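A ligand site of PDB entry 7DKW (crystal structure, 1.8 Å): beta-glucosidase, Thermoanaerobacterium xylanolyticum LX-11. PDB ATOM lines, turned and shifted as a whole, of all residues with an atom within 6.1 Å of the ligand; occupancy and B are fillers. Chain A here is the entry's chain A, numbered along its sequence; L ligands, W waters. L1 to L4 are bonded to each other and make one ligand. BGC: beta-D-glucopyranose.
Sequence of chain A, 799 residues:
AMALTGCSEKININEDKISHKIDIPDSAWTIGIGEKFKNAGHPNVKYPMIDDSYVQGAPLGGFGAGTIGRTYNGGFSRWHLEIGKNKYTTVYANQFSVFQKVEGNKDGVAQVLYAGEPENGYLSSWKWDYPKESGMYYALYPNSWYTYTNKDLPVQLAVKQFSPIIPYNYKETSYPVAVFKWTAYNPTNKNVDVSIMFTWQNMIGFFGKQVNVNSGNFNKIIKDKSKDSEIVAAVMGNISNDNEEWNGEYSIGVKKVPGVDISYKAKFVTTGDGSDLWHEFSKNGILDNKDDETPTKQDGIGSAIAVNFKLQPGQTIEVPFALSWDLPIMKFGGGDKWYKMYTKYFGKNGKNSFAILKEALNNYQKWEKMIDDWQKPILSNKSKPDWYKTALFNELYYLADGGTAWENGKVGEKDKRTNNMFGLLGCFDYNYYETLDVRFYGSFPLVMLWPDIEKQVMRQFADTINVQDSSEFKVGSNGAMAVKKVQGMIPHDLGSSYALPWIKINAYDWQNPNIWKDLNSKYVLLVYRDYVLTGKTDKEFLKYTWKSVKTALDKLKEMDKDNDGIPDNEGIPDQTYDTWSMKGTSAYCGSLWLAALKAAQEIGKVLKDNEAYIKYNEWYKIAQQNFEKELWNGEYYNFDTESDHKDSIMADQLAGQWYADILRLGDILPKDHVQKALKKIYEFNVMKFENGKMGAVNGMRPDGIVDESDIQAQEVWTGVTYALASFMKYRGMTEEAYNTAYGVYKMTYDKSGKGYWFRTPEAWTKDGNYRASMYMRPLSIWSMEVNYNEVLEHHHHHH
The side-chain carboxylate of Asp 578 is in hydrogen-bond range of an oxygen (O4) of BGC L4.
An oxygen (O3) of BGC L4 lies within hydrogen-bond range of the guanidinium group (NH1) of Arg 771, at 3.1 Å.
OH of Tyr 47 lies within hydrogen-bond range of O4 of BGC L3 (3.4 Å).
The side-chain amino group of Lys 46 sits at hydrogen-bond distance from an oxygen (O3) of BGC L1 (3.3 Å).
An oxygen (O3) of BGC L4 lies within hydrogen-bond range of the side-chain amide nitrogen of Gln 712 (3.5 Å).
CD1 of Tyr 430 touches C6 of BGC L4 (3.7 Å).
CE1 of Tyr 508 touches O4 of BGC L4, 3.5 Å away.
Trp 510 touches the ligand.
CG2 of Thr 579 touches O2 of BGC L4, at 3.5 Å.
Hydrophobic or aromatic side chains that line the ligand: Tyr 47, Tyr 430, Tyr 508 and Trp 510.
Of the 17 residues printed, 9 come within 4 Å of the ligand.
The nearest printed residue that does not touch the ligand is Tyr 432 (4.4 Å).
O of Arg 771 sits at hydrogen-bond distance from N of Glu 762.
OE1 of Gln 712 sits at hydrogen-bond distance from N of Thr 579 (3.0 Å).
The side-chain hydroxyl (OH) of Tyr 47 lies within hydrogen-bond range of the side-chain hydroxyl (OH) of Tyr 430, at 2.7 Å.
NE2 of Gln 712 lies within hydrogen-bond range of OD1 of Asp 578, at 3.1 Å.
OH of Tyr 430 is in hydrogen-bond range of NH1 of Arg 771 (3.1 Å).
The indole nitrogen (NE1) of Trp 510 sits at hydrogen-bond distance from the backbone carbonyl oxygen (O) of Asp 578, 3.4 Å away.
The side-chain carboxylate (OD2) of Asp 578 is in hydrogen-bond range of the side-chain hydroxyl (OH) of Tyr 508.
Water W6 lies within hydrogen-bond range of an oxygen (O2) of BGC L4 (2.6 Å), the side-chain hydroxyl (OG1) of Thr 579 (2.8 Å) and the side-chain amide nitrogen (NE2) of Gln 712 (3.1 Å).
Water W3 lies within hydrogen-bond range of an oxygen (O6) of BGC L4 (2.7 Å), the side-chain hydroxyl of Tyr 432 (2.8 Å), the side-chain carboxylate of Asp 509 (2.9 Å) and the backbone NH of Trp 510 (3.2 Å).
Water W1 bridges the side-chain hydroxyl of Tyr 47 (2.6 Å) and an oxygen (O2) of BGC L4 (2.9 Å).
Water W2 lies within hydrogen-bond range of OE2 of Glu 762 (2.8 Å), NH2 of Arg 771 (2.8 Å) and O3 of BGC L4 (3.2 Å).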
ATOM      1  N   LYS A  46      35.809  -1.149   3.695  1.00  0.00           N
ATOM      2  CA  LYS A  46      36.574  -0.796   4.931  1.00  0.00           C
ATOM      3  C   LYS A  46      35.765  -0.889   6.234  1.00  0.00           C
ATOM      4  O   LYS A  46      36.320  -0.973   7.319  1.00  0.00           O
ATOM      5  CB  LYS A  46      37.321   0.533   4.795  1.00  0.00           C
ATOM      6  CG  LYS A  46      36.499   1.761   4.395  1.00  0.00           C
ATOM      7  CD  LYS A  46      35.598   2.261   5.511  1.00  0.00           C
ATOM      8  CE  LYS A  46      35.263   3.742   5.304  1.00  0.00           C
ATOM      9  NZ  LYS A  46      36.342   4.675   5.743  1.00  0.00           N
ATOM     10  N   TYR A  47      34.448  -0.910   6.102  1.00  0.00           N
ATOM     11  CA  TYR A  47      33.529  -1.024   7.221  1.00  0.00           C
ATOM     12  C   TYR A  47      33.318  -2.507   7.531  1.00  0.00           C
ATOM     13  O   TYR A  47      33.554  -3.358   6.665  1.00  0.00           O
ATOM     14  CB  TYR A  47      32.214  -0.293   6.942  1.00  0.00           C
ATOM     15  CG  TYR A  47      31.461  -0.709   5.677  1.00  0.00           C
ATOM     16  CD1 TYR A  47      31.744  -0.116   4.447  1.00  0.00           C
ATOM     17  CD2 TYR A  47      30.416  -1.648   5.733  1.00  0.00           C
ATOM     18  CE1 TYR A  47      31.052  -0.487   3.301  1.00  0.00           C
ATOM     19  CE2 TYR A  47      29.700  -2.017   4.612  1.00  0.00           C
ATOM     20  CZ  TYR A  47      30.017  -1.460   3.385  1.00  0.00           C
ATOM     21  OH  TYR A  47      29.310  -1.839   2.263  1.00  0.00           O
ATOM     22  N   PRO A  48      32.896  -2.833   8.767  1.00  0.00           N
ATOM     23  CA  PRO A  48      32.798  -4.255   9.116  1.00  0.00           C
ATOM     24  C   PRO A  48      31.726  -4.968   8.314  1.00  0.00           C
ATOM     25  O   PRO A  48      30.707  -4.373   7.972  1.00  0.00           O
ATOM     26  CB  PRO A  48      32.451  -4.232  10.605  1.00  0.00           C
ATOM     27  CG  PRO A  48      32.941  -2.888  11.072  1.00  0.00           C
ATOM     28  CD  PRO A  48      32.601  -1.983   9.935  1.00  0.00           C
ATOM     29  N   TYR A 430      22.940  -5.660   5.070  1.00  0.00           N
ATOM     30  CA  TYR A 430      22.001  -4.582   4.783  1.00  0.00           C
ATOM     31  C   TYR A 430      20.631  -5.202   5.088  1.00  0.00           C
ATOM     32  O   TYR A 430      19.941  -5.718   4.202  1.00  0.00           O
ATOM     33  CB  TYR A 430      22.104  -4.102   3.333  1.00  0.00           C
ATOM     34  CG  TYR A 430      23.496  -3.933   2.779  1.00  0.00           C
ATOM     35  CD1 TYR A 430      24.521  -3.355   3.535  1.00  0.00           C
ATOM     36  CD2 TYR A 430      23.795  -4.329   1.464  1.00  0.00           C
ATOM     37  CE1 TYR A 430      25.789  -3.180   3.020  1.00  0.00           C
ATOM     38  CE2 TYR A 430      25.064  -4.154   0.949  1.00  0.00           C
ATOM     39  CZ  TYR A 430      26.061  -3.603   1.723  1.00  0.00           C
ATOM     40  OH  TYR A 430      27.326  -3.422   1.216  1.00  0.00           O
ATOM     41  N   TYR A 432      17.397  -5.585   5.508  1.00  0.00           N
ATOM     42  CA  TYR A 432      16.101  -5.016   5.101  1.00  0.00           C
ATOM     43  C   TYR A 432      15.256  -6.094   4.430  1.00  0.00           C
ATOM     44  O   TYR A 432      15.758  -6.827   3.572  1.00  0.00           O
ATOM     45  CB  TYR A 432      16.336  -3.852   4.144  1.00  0.00           C
ATOM     46  CG  TYR A 432      17.331  -2.835   4.708  1.00  0.00           C
ATOM     47  CD1 TYR A 432      17.112  -2.272   5.957  1.00  0.00           C
ATOM     48  CD2 TYR A 432      18.482  -2.467   3.998  1.00  0.00           C
ATOM     49  CE1 TYR A 432      18.016  -1.396   6.509  1.00  0.00           C
ATOM     50  CE2 TYR A 432      19.411  -1.559   4.553  1.00  0.00           C
ATOM     51  CZ  TYR A 432      19.145  -1.031   5.818  1.00  0.00           C
ATOM     52  OH  TYR A 432      19.981  -0.117   6.429  1.00  0.00           O
ATOM     53  N   HIS A 492      11.481   1.307  -0.398  1.00  0.00           N
ATOM     54  CA  HIS A 492      12.665   0.482  -0.605  1.00  0.00           C
ATOM     55  C   HIS A 492      12.519  -0.917  -0.006  1.00  0.00           C
ATOM     56  O   HIS A 492      12.955  -1.903  -0.612  1.00  0.00           O
ATOM     57  CB  HIS A 492      13.860   1.175   0.009  1.00  0.00           C
ATOM     58  CG  HIS A 492      15.136   0.427  -0.128  1.00  0.00           C
ATOM     59  ND1 HIS A 492      15.615  -0.385   0.879  1.00  0.00           N
ATOM     60  CD2 HIS A 492      16.066   0.391  -1.109  1.00  0.00           C
ATOM     61  CE1 HIS A 492      16.778  -0.893   0.517  1.00  0.00           C
ATOM     62  NE2 HIS A 492      17.070  -0.421  -0.674  1.00  0.00           N
ATOM     63  N   TYR A 508      15.981   1.249   5.276  1.00  0.00           N
ATOM     64  CA  TYR A 508      17.150   1.678   4.519  1.00  0.00           C
ATOM     65  C   TYR A 508      17.294   3.195   4.562  1.00  0.00           C
ATOM     66  O   TYR A 508      16.299   3.899   4.393  1.00  0.00           O
ATOM     67  CB  TYR A 508      17.042   1.174   3.067  1.00  0.00           C
ATOM     68  CG  TYR A 508      18.035   1.718   2.077  1.00  0.00           C
ATOM     69  CD1 TYR A 508      19.290   1.147   1.911  1.00  0.00           C
ATOM     70  CD2 TYR A 508      17.693   2.781   1.237  1.00  0.00           C
ATOM     71  CE1 TYR A 508      20.198   1.644   0.977  1.00  0.00           C
ATOM     72  CE2 TYR A 508      18.567   3.268   0.294  1.00  0.00           C
ATOM     73  CZ  TYR A 508      19.817   2.708   0.157  1.00  0.00           C
ATOM     74  OH  TYR A 508      20.711   3.239  -0.754  1.00  0.00           O
ATOM     75  N   ASP A 509      18.520   3.664   4.768  1.00  0.00           N
ATOM     76  CA  ASP A 509      18.785   5.110   4.880  1.00  0.00           C
ATOM     77  C   ASP A 509      20.037   5.637   4.187  1.00  0.00           C
ATOM     78  O   ASP A 509      20.360   6.812   4.361  1.00  0.00           O
ATOM     79  CB  ASP A 509      18.761   5.538   6.361  1.00  0.00           C
ATOM     80  CG  ASP A 509      19.873   4.905   7.197  1.00  0.00           C
ATOM     81  OD1 ASP A 509      20.813   4.289   6.643  1.00  0.00           O
ATOM     82  OD2 ASP A 509      19.797   5.033   8.428  1.00  0.00           O
ATOM     83  N   TRP A 510      20.741   4.821   3.408  1.00  0.00           N
ATOM     84  CA  TRP A 510      21.986   5.289   2.754  1.00  0.00           C
ATOM     85  C   TRP A 510      21.711   6.378   1.718  1.00  0.00           C
ATOM     86  O   TRP A 510      22.519   7.308   1.525  1.00  0.00           O
ATOM     87  CB  TRP A 510      22.749   4.120   2.082  1.00  0.00           C
ATOM     88  CG  TRP A 510      23.974   4.591   1.402  1.00  0.00           C
ATOM     89  CD1 TRP A 510      24.203   4.617   0.058  1.00  0.00           C
ATOM     90  CD2 TRP A 510      25.139   5.170   2.015  1.00  0.00           C
ATOM     91  NE1 TRP A 510      25.448   5.145  -0.190  1.00  0.00           N
ATOM     92  CE2 TRP A 510      26.038   5.497   0.987  1.00  0.00           C
ATOM     93  CE3 TRP A 510      25.498   5.428   3.343  1.00  0.00           C
ATOM     94  CZ2 TRP A 510      27.279   6.091   1.231  1.00  0.00           C
ATOM     95  CZ3 TRP A 510      26.739   6.021   3.587  1.00  0.00           C
ATOM     96  CH2 TRP A 510      27.619   6.334   2.533  1.00  0.00           C
ATOM     97  N   THR A 576      18.958   1.357  -7.585  1.00  0.00           N
ATOM     98  CA  THR A 576      19.653   0.200  -6.967  1.00  0.00           C
ATOM     99  C   THR A 576      21.174   0.313  -6.917  1.00  0.00           C
ATOM    100  O   THR A 576      21.803  -0.152  -5.963  1.00  0.00           O
ATOM    101  CB  THR A 576      19.233  -1.141  -7.652  1.00  0.00           C
ATOM    102  OG1 THR A 576      19.410  -2.249  -6.729  1.00  0.00           O
ATOM    103  CG2 THR A 576      20.012  -1.390  -8.913  1.00  0.00           C
ATOM    104  N   ASP A 578      23.363   2.209  -5.780  1.00  0.00           N
ATOM    105  CA  ASP A 578      23.192   3.314  -4.837  1.00  0.00           C
ATOM    106  C   ASP A 578      24.464   4.017  -4.364  1.00  0.00           C
ATOM    107  O   ASP A 578      24.396   4.804  -3.436  1.00  0.00           O
ATOM    108  CB  ASP A 578      22.317   2.856  -3.652  1.00  0.00           C
ATOM    109  CG  ASP A 578      22.998   1.857  -2.742  1.00  0.00           C
ATOM    110  OD1 ASP A 578      24.012   1.264  -3.144  1.00  0.00           O
ATOM    111  OD2 ASP A 578      22.493   1.659  -1.611  1.00  0.00           O
ATOM    112  N   THR A 579      25.601   3.749  -5.013  1.00  0.00           N
ATOM    113  CA  THR A 579      26.756   4.662  -4.971  1.00  0.00           C
ATOM    114  C   THR A 579      27.189   5.152  -6.371  1.00  0.00           C
ATOM    115  O   THR A 579      28.121   5.936  -6.478  1.00  0.00           O
ATOM    116  CB  THR A 579      27.992   4.092  -4.198  1.00  0.00           C
ATOM    117  OG1 THR A 579      28.471   2.885  -4.798  1.00  0.00           O
ATOM    118  CG2 THR A 579      27.646   3.830  -2.731  1.00  0.00           C
ATOM    119  N   ILE A 711      33.086   2.531  -7.329  1.00  0.00           N
ATOM    120  CA  ILE A 711      33.282   1.120  -6.989  1.00  0.00           C
ATOM    121  C   ILE A 711      32.257   0.192  -7.643  1.00  0.00           C
ATOM    122  O   ILE A 711      32.634  -0.872  -8.132  1.00  0.00           O
ATOM    123  CB  ILE A 711      33.336   0.900  -5.461  1.00  0.00           C
ATOM    124  CG1 ILE A 711      33.744  -0.547  -5.123  1.00  0.00           C
ATOM    125  CG2 ILE A 711      32.000   1.235  -4.798  1.00  0.00           C
ATOM    126  CD1 ILE A 711      35.048  -0.991  -5.764  1.00  0.00           C
ATOM    127  N   GLN A 712      30.986   0.580  -7.685  1.00  0.00           N
ATOM    128  CA  GLN A 712      29.956  -0.296  -8.247  1.00  0.00           C
ATOM    129  C   GLN A 712      30.124  -0.570  -9.739  1.00  0.00           C
ATOM    130  O   GLN A 712      29.749  -1.642 -10.222  1.00  0.00           O
ATOM    131  CB  GLN A 712      28.548   0.226  -7.950  1.00  0.00           C
ATOM    132  CG  GLN A 712      28.225   0.118  -6.476  1.00  0.00           C
ATOM    133  CD  GLN A 712      26.862   0.664  -6.107  1.00  0.00           C
ATOM    134  OE1 GLN A 712      26.291   1.511  -6.814  1.00  0.00           O
ATOM    135  NE2 GLN A 712      26.345   0.232  -4.961  1.00  0.00           N
ATOM    136  N   TRP A 717      28.006  -7.791 -10.380  1.00  0.00           N
ATOM    137  CA  TRP A 717      26.863  -8.140  -9.522  1.00  0.00           C
ATOM    138  C   TRP A 717      26.318  -9.497  -9.980  1.00  0.00           C
ATOM    139  O   TRP A 717      25.872  -9.673 -11.118  1.00  0.00           O
ATOM    140  CB  TRP A 717      25.796  -7.067  -9.539  1.00  0.00           C
ATOM    141  CG  TRP A 717      26.179  -5.847  -8.760  1.00  0.00           C
ATOM    142  CD1 TRP A 717      27.439  -5.489  -8.327  1.00  0.00           C
ATOM    143  CD2 TRP A 717      25.312  -4.814  -8.319  1.00  0.00           C
ATOM    144  NE1 TRP A 717      27.385  -4.305  -7.632  1.00  0.00           N
ATOM    145  CE2 TRP A 717      26.086  -3.863  -7.621  1.00  0.00           C
ATOM    146  CE3 TRP A 717      23.935  -4.593  -8.441  1.00  0.00           C
ATOM    147  CZ2 TRP A 717      25.532  -2.712  -7.043  1.00  0.00           C
ATOM    148  CZ3 TRP A 717      23.370  -3.444  -7.855  1.00  0.00           C
ATOM    149  CH2 TRP A 717      24.169  -2.535  -7.166  1.00  0.00           C
ATOM    150  N   GLU A 762      26.400 -10.217  -3.203  1.00  0.00           N
ATOM    151  CA  GLU A 762      26.002  -9.226  -4.204  1.00  0.00           C
ATOM    152  C   GLU A 762      27.076  -9.138  -5.282  1.00  0.00           C
ATOM    153  O   GLU A 762      26.780  -9.229  -6.458  1.00  0.00           O
ATOM    154  CB  GLU A 762      25.819  -7.850  -3.538  1.00  0.00           C
ATOM    155  CG  GLU A 762      25.684  -6.660  -4.497  1.00  0.00           C
ATOM    156  CD  GLU A 762      24.277  -6.439  -4.951  1.00  0.00           C
ATOM    157  OE1 GLU A 762      23.768  -7.239  -5.771  1.00  0.00           O
ATOM    158  OE2 GLU A 762      23.645  -5.462  -4.487  1.00  0.00           O
ATOM    159  N   ARG A 771      31.503  -8.230  -1.751  1.00  0.00           N
ATOM    160  CA  ARG A 771      30.664  -7.378  -0.931  1.00  0.00           C
ATOM    161  C   ARG A 771      29.285  -8.024  -0.732  1.00  0.00           C
ATOM    162  O   ARG A 771      28.637  -8.424  -1.706  1.00  0.00           O
ATOM    163  CB  ARG A 771      30.518  -5.996  -1.543  1.00  0.00           C
ATOM    164  CG  ARG A 771      29.744  -5.002  -0.687  1.00  0.00           C
ATOM    165  CD  ARG A 771      29.844  -3.593  -1.250  1.00  0.00           C
ATOM    166  NE  ARG A 771      29.240  -3.441  -2.566  1.00  0.00           N
ATOM    167  CZ  ARG A 771      27.952  -3.237  -2.829  1.00  0.00           C
ATOM    168  NH1 ARG A 771      27.043  -3.169  -1.873  1.00  0.00           N
ATOM    169  NH2 ARG A 771      27.562  -3.125  -4.089  1.00  0.00           N
HETATM  170  C2  BGC L   1      36.497   8.910   9.136  1.00  0.00           C
HETATM  171  C3  BGC L   1      36.268   8.035   7.926  1.00  0.00           C
HETATM  172  C4  BGC L   1      34.961   8.439   7.274  1.00  0.00           C
HETATM  173  C5  BGC L   1      35.035   9.921   6.884  1.00  0.00           C
HETATM  174  C6  BGC L   1      33.875  10.455   6.029  1.00  0.00           C
HETATM  175  C1  BGC L   1      36.293  10.402   8.866  1.00  0.00           C
HETATM  176  O1  BGC L   1      36.173  11.095  10.112  1.00  0.00           O
HETATM  177  O2  BGC L   1      37.834   8.655   9.565  1.00  0.00           O
HETATM  178  O3  BGC L   1      36.246   6.659   8.319  1.00  0.00           O
HETATM  179  O4  BGC L   1      34.765   7.616   6.136  1.00  0.00           O
HETATM  180  O5  BGC L   1      35.093  10.645   8.117  1.00  0.00           O
HETATM  181  O6  BGC L   1      32.589  10.225   6.626  1.00  0.00           O
HETATM  182  C2  BGC L   2      33.091   6.831   4.652  1.00  0.00           C
HETATM  183  C3  BGC L   2      31.700   6.206   4.567  1.00  0.00           C
HETATM  184  C4  BGC L   2      31.573   5.033   5.544  1.00  0.00           C
HETATM  185  C5  BGC L   2      32.014   5.412   6.971  1.00  0.00           C
HETATM  186  C6  BGC L   2      31.913   4.243   7.958  1.00  0.00           C
HETATM  187  C1  BGC L   2      33.439   7.093   6.103  1.00  0.00           C
HETATM  188  O2  BGC L   2      33.107   8.059   3.898  1.00  0.00           O
HETATM  189  O3  BGC L   2      31.546   5.795   3.198  1.00  0.00           O
HETATM  190  O4  BGC L   2      30.221   4.612   5.598  1.00  0.00           O
HETATM  191  O5  BGC L   2      33.359   5.932   6.936  1.00  0.00           O
HETATM  192  O6  BGC L   2      32.744   3.142   7.574  1.00  0.00           O
HETATM  193  C2  BGC L   3      28.541   2.968   5.258  1.00  0.00           C
HETATM  194  C3  BGC L   3      28.031   1.893   4.302  1.00  0.00           C
HETATM  195  C4  BGC L   3      28.123   2.337   2.833  1.00  0.00           C
HETATM  196  C5  BGC L   3      29.511   2.873   2.492  1.00  0.00           C
HETATM  197  C6  BGC L   3      29.623   3.325   1.027  1.00  0.00           C
HETATM  198  C1  BGC L   3      29.894   3.487   4.780  1.00  0.00           C
HETATM  199  O2  BGC L   3      28.643   2.427   6.601  1.00  0.00           O
HETATM  200  O3  BGC L   3      26.690   1.545   4.653  1.00  0.00           O
HETATM  201  O4  BGC L   3      27.862   1.209   1.983  1.00  0.00           O
HETATM  202  O5  BGC L   3      29.854   3.913   3.417  1.00  0.00           O
HETATM  203  O6  BGC L   3      30.914   3.894   0.785  1.00  0.00           O
HETATM  204  C2  BGC L   4      26.687   0.350   0.098  1.00  0.00           C
HETATM  205  C3  BGC L   4      25.325   0.297  -0.549  1.00  0.00           C
HETATM  206  C4  BGC L   4      24.296  -0.187   0.474  1.00  0.00           C
HETATM  207  C5  BGC L   4      24.333   0.679   1.728  1.00  0.00           C
HETATM  208  C6  BGC L   4      23.405   0.127   2.809  1.00  0.00           C
HETATM  209  C1  BGC L   4      26.609   1.230   1.326  1.00  0.00           C
HETATM  210  O2  BGC L   4      27.596   0.917  -0.845  1.00  0.00           O
HETATM  211  O3  BGC L   4      25.355  -0.536  -1.713  1.00  0.00           O
HETATM  212  O4  BGC L   4      22.981  -0.198  -0.073  1.00  0.00           O
HETATM  213  O5  BGC L   4      25.644   0.736   2.268  1.00  0.00           O
HETATM  214  O6  BGC L   4      23.437   0.980   3.964  1.00  0.00           O
HETATM  215  O   HOH W   1      29.973  -0.307   0.254  1.00  0.00           O
HETATM  216  O   HOH W   2      24.749  -3.020  -3.701  1.00  0.00           O
HETATM  217  O   HOH W   3      21.123   1.988   4.950  1.00  0.00           O
HETATM  218  O   HOH W   4      33.055   2.933   2.835  1.00  0.00           O
HETATM  219  O   HOH W   5      30.627   6.276  -0.088  1.00  0.00           O
HETATM  220  O   HOH W   6      28.792   0.592  -3.153  1.00  0.00           O
